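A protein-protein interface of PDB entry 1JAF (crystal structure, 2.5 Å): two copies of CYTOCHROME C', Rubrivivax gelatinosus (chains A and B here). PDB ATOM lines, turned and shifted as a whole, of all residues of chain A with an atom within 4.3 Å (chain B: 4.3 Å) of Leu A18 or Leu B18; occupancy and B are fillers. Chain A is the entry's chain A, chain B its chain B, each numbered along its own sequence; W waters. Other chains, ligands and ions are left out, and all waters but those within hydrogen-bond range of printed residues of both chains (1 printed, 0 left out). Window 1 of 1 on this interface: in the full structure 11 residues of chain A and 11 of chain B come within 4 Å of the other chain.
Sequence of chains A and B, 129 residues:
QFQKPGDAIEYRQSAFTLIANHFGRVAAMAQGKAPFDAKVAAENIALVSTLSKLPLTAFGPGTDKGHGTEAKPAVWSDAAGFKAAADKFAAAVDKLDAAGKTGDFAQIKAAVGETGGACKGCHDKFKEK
Among the printed residues, pairs that only touch across the chains: Leu A18 with Tyr B11, Ser A14 with Ser B14, Thr A17 with Ser B14, Tyr A11 with Leu B18, Leu A18 with Leu B18, Asn A21 with Tyr B11, Ser A14 with Thr B17, Tyr A11 with Asn B21, Leu A51 with Leu B51 and Leu A18 with Leu B51.
The side-chain hydroxyl of Tyr A11 sits at hydrogen-bond distance from a ring nitrogen (NE2) of His B22 (2.8 Å).
The side-chain hydroxyl (OH) of Tyr B11 lies within hydrogen-bond range of a ring nitrogen (NE2) of His A22, at 2.6 Å.
Of chain B, only Tyr B11 (3.4 Å), Leu B18 (3.8 Å) and Leu B51 (3.9 Å) come within 4 Å of Leu A18.
Printed residues of chain B within 4 Å of His A22: Tyr B11.
Of the printed residues of chain A, Ser B14 touches Ser A14 (3.5 Å) and Thr A17 (3.5 Å).
Of chain A, only Tyr A11 (3.6 Å) and Leu A18 (3.8 Å) come within 4 Å of Leu B18.
Of the printed residues of chain A, Asn B21 touches Tyr A11.
The nearest residue of chain B that does not touch Leu A18 is Ala B15 (4.2 Å).
The nearest residue of chain A that does not touch Leu B18 is Ala A15 (4.02 Å).
The nearest printed residue of chain B that does not touch Leu A51 is Leu B18 (4.1 Å).
Tyr A11 touches Leu B18, and with the chains exchanged Leu A18 touches Tyr B11.
Tyr A11 touches Asn B21, and with the chains exchanged Asn A21 touches Tyr B11.
Tyr A11 touches His B22, and with the chains exchanged His A22 touches Tyr B11.
Leu A18 touches Leu B51, but with the chains exchanged Leu A51 does not touch Leu B18 (4.1 Å).
Of the 12 pairs that touch across the chains among the printed residues, 11 have their exchanged pair printed and touching as well.
Water W1 lies within hydrogen-bond range of OG of Ser B14 (2.9 Å) and OG1 of Thr A17 (3.2 Å).
Of the 11 printed residues of chain B, 7 touch a printed residue of chain A.
Printed residues of chain B that touch a printed residue of chain A: Tyr B11, Ser B14, Thr B17, Leu B18, Asn B21, His B22 and Leu B51.
Hydrophobic or aromatic side chains of chain B within 4 Å of the printed part of chain A: Tyr B11, Leu B18, His B22 and Leu B51.
Printed residues of chain A that touch a printed residue of chain B: Tyr A11, Ser A14, Thr A17, Leu A18, Asn A21, His A22 and Leu A51.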
ATOM      1  N   TYR A  11      23.365 -16.712  13.942  1.00  0.00           N
ATOM      2  CA  TYR A  11      23.589 -17.342  15.238  1.00  0.00           C
ATOM      3  C   TYR A  11      22.449 -18.288  15.580  1.00  0.00           C
ATOM      4  O   TYR A  11      22.671 -19.446  15.933  1.00  0.00           O
ATOM      5  CB  TYR A  11      23.688 -16.271  16.317  1.00  0.00           C
ATOM      6  CG  TYR A  11      23.856 -16.814  17.707  1.00  0.00           C
ATOM      7  CD1 TYR A  11      25.119 -17.102  18.203  1.00  0.00           C
ATOM      8  CD2 TYR A  11      22.758 -17.016  18.547  1.00  0.00           C
ATOM      9  CE1 TYR A  11      25.285 -17.571  19.498  1.00  0.00           C
ATOM     10  CE2 TYR A  11      22.922 -17.490  19.850  1.00  0.00           C
ATOM     11  CZ  TYR A  11      24.190 -17.759  20.313  1.00  0.00           C
ATOM     12  OH  TYR A  11      24.392 -18.188  21.597  1.00  0.00           O
ATOM     13  N   SER A  14      22.246 -21.389  13.221  1.00  0.00           N
ATOM     14  CA  SER A  14      23.299 -22.337  13.532  1.00  0.00           C
ATOM     15  C   SER A  14      22.965 -23.121  14.778  1.00  0.00           C
ATOM     16  O   SER A  14      23.209 -24.329  14.846  1.00  0.00           O
ATOM     17  CB  SER A  14      24.600 -21.590  13.708  1.00  0.00           C
ATOM     18  OG  SER A  14      24.854 -20.846  12.538  1.00  0.00           O
ATOM     19  N   ALA A  15      22.413 -22.442  15.775  1.00  0.00           N
ATOM     20  CA  ALA A  15      22.037 -23.118  17.009  1.00  0.00           C
ATOM     21  C   ALA A  15      20.956 -24.155  16.722  1.00  0.00           C
ATOM     22  O   ALA A  15      21.059 -25.295  17.162  1.00  0.00           O
ATOM     23  CB  ALA A  15      21.557 -22.121  18.019  1.00  0.00           C
ATOM     24  N   PHE A  16      19.940 -23.791  15.948  1.00  0.00           N
ATOM     25  CA  PHE A  16      18.882 -24.744  15.621  1.00  0.00           C
ATOM     26  C   PHE A  16      19.432 -25.928  14.869  1.00  0.00           C
ATOM     27  O   PHE A  16      19.070 -27.064  15.152  1.00  0.00           O
ATOM     28  CB  PHE A  16      17.772 -24.078  14.832  1.00  0.00           C
ATOM     29  CG  PHE A  16      16.881 -23.235  15.671  1.00  0.00           C
ATOM     30  CD1 PHE A  16      16.365 -23.742  16.853  1.00  0.00           C
ATOM     31  CD2 PHE A  16      16.574 -21.933  15.307  1.00  0.00           C
ATOM     32  CE1 PHE A  16      15.543 -22.967  17.672  1.00  0.00           C
ATOM     33  CE2 PHE A  16      15.757 -21.149  16.108  1.00  0.00           C
ATOM     34  CZ  PHE A  16      15.236 -21.666  17.306  1.00  0.00           C
ATOM     35  N   THR A  17      20.346 -25.681  13.947  1.00  0.00           N
ATOM     36  CA  THR A  17      20.965 -26.751  13.181  1.00  0.00           C
ATOM     37  C   THR A  17      21.667 -27.760  14.109  1.00  0.00           C
ATOM     38  O   THR A  17      21.525 -28.979  13.929  1.00  0.00           O
ATOM     39  CB  THR A  17      21.989 -26.167  12.199  1.00  0.00           C
ATOM     40  OG1 THR A  17      21.319 -25.291  11.287  1.00  0.00           O
ATOM     41  CG2 THR A  17      22.695 -27.253  11.419  1.00  0.00           C
ATOM     42  N   LEU A  18      22.380 -27.273  15.125  1.00  0.00           N
ATOM     43  CA  LEU A  18      23.071 -28.194  16.029  1.00  0.00           C
ATOM     44  C   LEU A  18      22.079 -28.950  16.890  1.00  0.00           C
ATOM     45  O   LEU A  18      22.249 -30.146  17.111  1.00  0.00           O
ATOM     46  CB  LEU A  18      24.106 -27.489  16.920  1.00  0.00           C
ATOM     47  CG  LEU A  18      25.391 -26.893  16.328  1.00  0.00           C
ATOM     48  CD1 LEU A  18      26.334 -26.564  17.460  1.00  0.00           C
ATOM     49  CD2 LEU A  18      26.069 -27.863  15.409  1.00  0.00           C
ATOM     50  N   ILE A  19      21.045 -28.262  17.366  1.00  0.00           N
ATOM     51  CA  ILE A  19      20.006 -28.871  18.194  1.00  0.00           C
ATOM     52  C   ILE A  19      19.305 -29.966  17.408  1.00  0.00           C
ATOM     53  O   ILE A  19      19.080 -31.075  17.900  1.00  0.00           O
ATOM     54  CB  ILE A  19      18.965 -27.823  18.603  1.00  0.00           C
ATOM     55  CG1 ILE A  19      19.581 -26.872  19.626  1.00  0.00           C
ATOM     56  CG2 ILE A  19      17.740 -28.488  19.172  1.00  0.00           C
ATOM     57  CD1 ILE A  19      18.714 -25.686  19.957  1.00  0.00           C
ATOM     58  N   ALA A  20      18.959 -29.663  16.171  1.00  0.00           N
ATOM     59  CA  ALA A  20      18.299 -30.649  15.335  1.00  0.00           C
ATOM     60  C   ALA A  20      19.167 -31.886  15.210  1.00  0.00           C
ATOM     61  O   ALA A  20      18.715 -32.999  15.471  1.00  0.00           O
ATOM     62  CB  ALA A  20      18.017 -30.074  13.959  1.00  0.00           C
ATOM     63  N   ASN A  21      20.440 -31.711  14.884  1.00  0.00           N
ATOM     64  CA  ASN A  21      21.297 -32.869  14.703  1.00  0.00           C
ATOM     65  C   ASN A  21      21.418 -33.756  15.934  1.00  0.00           C
ATOM     66  O   ASN A  21      21.224 -34.955  15.858  1.00  0.00           O
ATOM     67  CB  ASN A  21      22.682 -32.469  14.198  1.00  0.00           C
ATOM     68  CG  ASN A  21      23.490 -33.667  13.745  1.00  0.00           C
ATOM     69  OD1 ASN A  21      24.084 -34.377  14.555  1.00  0.00           O
ATOM     70  ND2 ASN A  21      23.507 -33.905  12.442  1.00  0.00           N
ATOM     71  N   HIS A  22      21.680 -33.154  17.080  1.00  0.00           N
ATOM     72  CA  HIS A  22      21.843 -33.936  18.295  1.00  0.00           C
ATOM     73  C   HIS A  22      20.537 -34.487  18.853  1.00  0.00           C
ATOM     74  O   HIS A  22      20.540 -35.536  19.498  1.00  0.00           O
ATOM     75  CB  HIS A  22      22.605 -33.122  19.353  1.00  0.00           C
ATOM     76  CG  HIS A  22      24.083 -32.895  19.006  1.00  0.00           C
ATOM     77  ND1 HIS A  22      25.048 -33.872  19.196  1.00  0.00           N
ATOM     78  CD2 HIS A  22      24.616 -31.797  18.337  1.00  0.00           C
ATOM     79  CE1 HIS A  22      26.150 -33.360  18.627  1.00  0.00           C
ATOM     80  NE2 HIS A  22      25.947 -32.184  18.148  1.00  0.00           N
ATOM     81  N   LEU A  51      22.350 -26.132  24.480  1.00  0.00           N
ATOM     82  CA  LEU A  51      22.078 -25.319  23.305  1.00  0.00           C
ATOM     83  C   LEU A  51      20.672 -24.715  23.236  1.00  0.00           C
ATOM     84  O   LEU A  51      20.492 -23.645  22.656  1.00  0.00           O
ATOM     85  CB  LEU A  51      22.354 -26.139  22.038  1.00  0.00           C
ATOM     86  CG  LEU A  51      23.766 -26.698  21.851  1.00  0.00           C
ATOM     87  CD1 LEU A  51      23.787 -27.746  20.761  1.00  0.00           C
ATOM     88  CD2 LEU A  51      24.716 -25.574  21.518  1.00  0.00           C
ATOM     89  N   TYR B  11      26.586 -28.447   9.523  1.00  0.00           N
ATOM     90  CA  TYR B  11      26.830 -28.684  10.925  1.00  0.00           C
ATOM     91  C   TYR B  11      28.133 -28.024  11.354  1.00  0.00           C
ATOM     92  O   TYR B  11      28.155 -27.238  12.302  1.00  0.00           O
ATOM     93  CB  TYR B  11      26.873 -30.185  11.183  1.00  0.00           C
ATOM     94  CG  TYR B  11      27.117 -30.573  12.617  1.00  0.00           C
ATOM     95  CD1 TYR B  11      28.413 -30.726  13.094  1.00  0.00           C
ATOM     96  CD2 TYR B  11      26.058 -30.835  13.489  1.00  0.00           C
ATOM     97  CE1 TYR B  11      28.656 -31.132  14.385  1.00  0.00           C
ATOM     98  CE2 TYR B  11      26.300 -31.246  14.796  1.00  0.00           C
ATOM     99  CZ  TYR B  11      27.607 -31.396  15.230  1.00  0.00           C
ATOM    100  OH  TYR B  11      27.896 -31.846  16.493  1.00  0.00           O
ATOM    101  N   SER B  14      27.914 -24.279  11.302  1.00  0.00           N
ATOM    102  CA  SER B  14      27.101 -23.800  12.412  1.00  0.00           C
ATOM    103  C   SER B  14      27.895 -23.862  13.722  1.00  0.00           C
ATOM    104  O   SER B  14      27.775 -22.986  14.568  1.00  0.00           O
ATOM    105  CB  SER B  14      25.812 -24.619  12.530  1.00  0.00           C
ATOM    106  OG  SER B  14      25.005 -24.503  11.369  1.00  0.00           O
ATOM    107  N   ALA B  15      28.713 -24.885  13.896  1.00  0.00           N
ATOM    108  CA  ALA B  15      29.497 -24.987  15.115  1.00  0.00           C
ATOM    109  C   ALA B  15      30.536 -23.861  15.202  1.00  0.00           C
ATOM    110  O   ALA B  15      30.677 -23.208  16.236  1.00  0.00           O
ATOM    111  CB  ALA B  15      30.173 -26.335  15.175  1.00  0.00           C
ATOM    112  N   PHE B  16      31.250 -23.610  14.113  1.00  0.00           N
ATOM    113  CA  PHE B  16      32.240 -22.560  14.118  1.00  0.00           C
ATOM    114  C   PHE B  16      31.625 -21.217  14.390  1.00  0.00           C
ATOM    115  O   PHE B  16      32.238 -20.387  15.042  1.00  0.00           O
ATOM    116  CB  PHE B  16      33.003 -22.533  12.818  1.00  0.00           C
ATOM    117  CG  PHE B  16      34.011 -23.625  12.700  1.00  0.00           C
ATOM    118  CD1 PHE B  16      34.949 -23.816  13.708  1.00  0.00           C
ATOM    119  CD2 PHE B  16      34.026 -24.476  11.595  1.00  0.00           C
ATOM    120  CE1 PHE B  16      35.892 -24.842  13.613  1.00  0.00           C
ATOM    121  CE2 PHE B  16      34.974 -25.511  11.494  1.00  0.00           C
ATOM    122  CZ  PHE B  16      35.903 -25.692  12.502  1.00  0.00           C
ATOM    123  N   THR B  17      30.412 -20.990  13.910  1.00  0.00           N
ATOM    124  CA  THR B  17      29.733 -19.723  14.136  1.00  0.00           C
ATOM    125  C   THR B  17      29.422 -19.514  15.611  1.00  0.00           C
ATOM    126  O   THR B  17      29.633 -18.424  16.150  1.00  0.00           O
ATOM    127  CB  THR B  17      28.429 -19.659  13.337  1.00  0.00           C
ATOM    128  OG1 THR B  17      28.733 -19.600  11.940  1.00  0.00           O
ATOM    129  CG2 THR B  17      27.595 -18.451  13.707  1.00  0.00           C
ATOM    130  N   LEU B  18      28.933 -20.549  16.282  1.00  0.00           N
ATOM    131  CA  LEU B  18      28.605 -20.420  17.690  1.00  0.00           C
ATOM    132  C   LEU B  18      29.885 -20.206  18.463  1.00  0.00           C
ATOM    133  O   LEU B  18      29.947 -19.333  19.315  1.00  0.00           O
ATOM    134  CB  LEU B  18      27.863 -21.652  18.206  1.00  0.00           C
ATOM    135  CG  LEU B  18      26.456 -21.908  17.642  1.00  0.00           C
ATOM    136  CD1 LEU B  18      25.772 -22.948  18.490  1.00  0.00           C
ATOM    137  CD2 LEU B  18      25.625 -20.659  17.640  1.00  0.00           C
ATOM    138  N   ILE B  19      30.915 -20.971  18.129  1.00  0.00           N
ATOM    139  CA  ILE B  19      32.215 -20.860  18.785  1.00  0.00           C
ATOM    140  C   ILE B  19      32.764 -19.448  18.621  1.00  0.00           C
ATOM    141  O   ILE B  19      33.157 -18.798  19.590  1.00  0.00           O
ATOM    142  CB  ILE B  19      33.218 -21.853  18.171  1.00  0.00           C
ATOM    143  CG1 ILE B  19      32.823 -23.276  18.551  1.00  0.00           C
ATOM    144  CG2 ILE B  19      34.638 -21.545  18.611  1.00  0.00           C
ATOM    145  CD1 ILE B  19      33.629 -24.334  17.836  1.00  0.00           C
ATOM    146  N   ALA B  20      32.737 -18.945  17.397  1.00  0.00           N
ATOM    147  CA  ALA B  20      33.235 -17.614  17.123  1.00  0.00           C
ATOM    148  C   ALA B  20      32.545 -16.573  17.989  1.00  0.00           C
ATOM    149  O   ALA B  20      33.189 -15.724  18.608  1.00  0.00           O
ATOM    150  CB  ALA B  20      33.036 -17.289  15.676  1.00  0.00           C
ATOM    151  N   ASN B  21      31.233 -16.653  18.078  1.00  0.00           N
ATOM    152  CA  ASN B  21      30.482 -15.684  18.847  1.00  0.00           C
ATOM    153  C   ASN B  21      30.809 -15.688  20.333  1.00  0.00           C
ATOM    154  O   ASN B  21      31.026 -14.638  20.917  1.00  0.00           O
ATOM    155  CB  ASN B  21      28.992 -15.894  18.639  1.00  0.00           C
ATOM    156  CG  ASN B  21      28.185 -14.752  19.156  1.00  0.00           C
ATOM    157  OD1 ASN B  21      27.805 -14.733  20.324  1.00  0.00           O
ATOM    158  ND2 ASN B  21      27.903 -13.782  18.288  1.00  0.00           N
ATOM    159  N   HIS B  22      30.845 -16.859  20.944  1.00  0.00           N
ATOM    160  CA  HIS B  22      31.125 -16.937  22.366  1.00  0.00           C
ATOM    161  C   HIS B  22      32.581 -16.657  22.672  1.00  0.00           C
ATOM    162  O   HIS B  22      32.905 -16.033  23.670  1.00  0.00           O
ATOM    163  CB  HIS B  22      30.721 -18.299  22.921  1.00  0.00           C
ATOM    164  CG  HIS B  22      29.207 -18.275  22.942  1.00  0.00           C
ATOM    165  ND1 HIS B  22      28.440 -17.683  23.933  1.00  0.00           N
ATOM    166  CD2 HIS B  22      28.387 -18.744  21.921  1.00  0.00           C
ATOM    167  CE1 HIS B  22      27.161 -17.765  23.514  1.00  0.00           C
ATOM    168  NE2 HIS B  22      27.104 -18.386  22.376  1.00  0.00           N
ATOM    169  N   LEU B  51      31.557 -26.819  22.693  1.00  0.00           N
ATOM    170  CA  LEU B  51      31.390 -26.735  21.242  1.00  0.00           C
ATOM    171  C   LEU B  51      32.620 -27.076  20.432  1.00  0.00           C
ATOM    172  O   LEU B  51      32.493 -27.587  19.323  1.00  0.00           O
ATOM    173  CB  LEU B  51      30.943 -25.333  20.829  1.00  0.00           C
ATOM    174  CG  LEU B  51      29.592 -24.788  21.283  1.00  0.00           C
ATOM    175  CD1 LEU B  51      29.515 -23.312  21.022  1.00  0.00           C
ATOM    176  CD2 LEU B  51      28.494 -25.495  20.555  1.00  0.00           C
HETATM  177  O   HOH W   1      23.121 -23.324   9.463  1.00  0.00           O
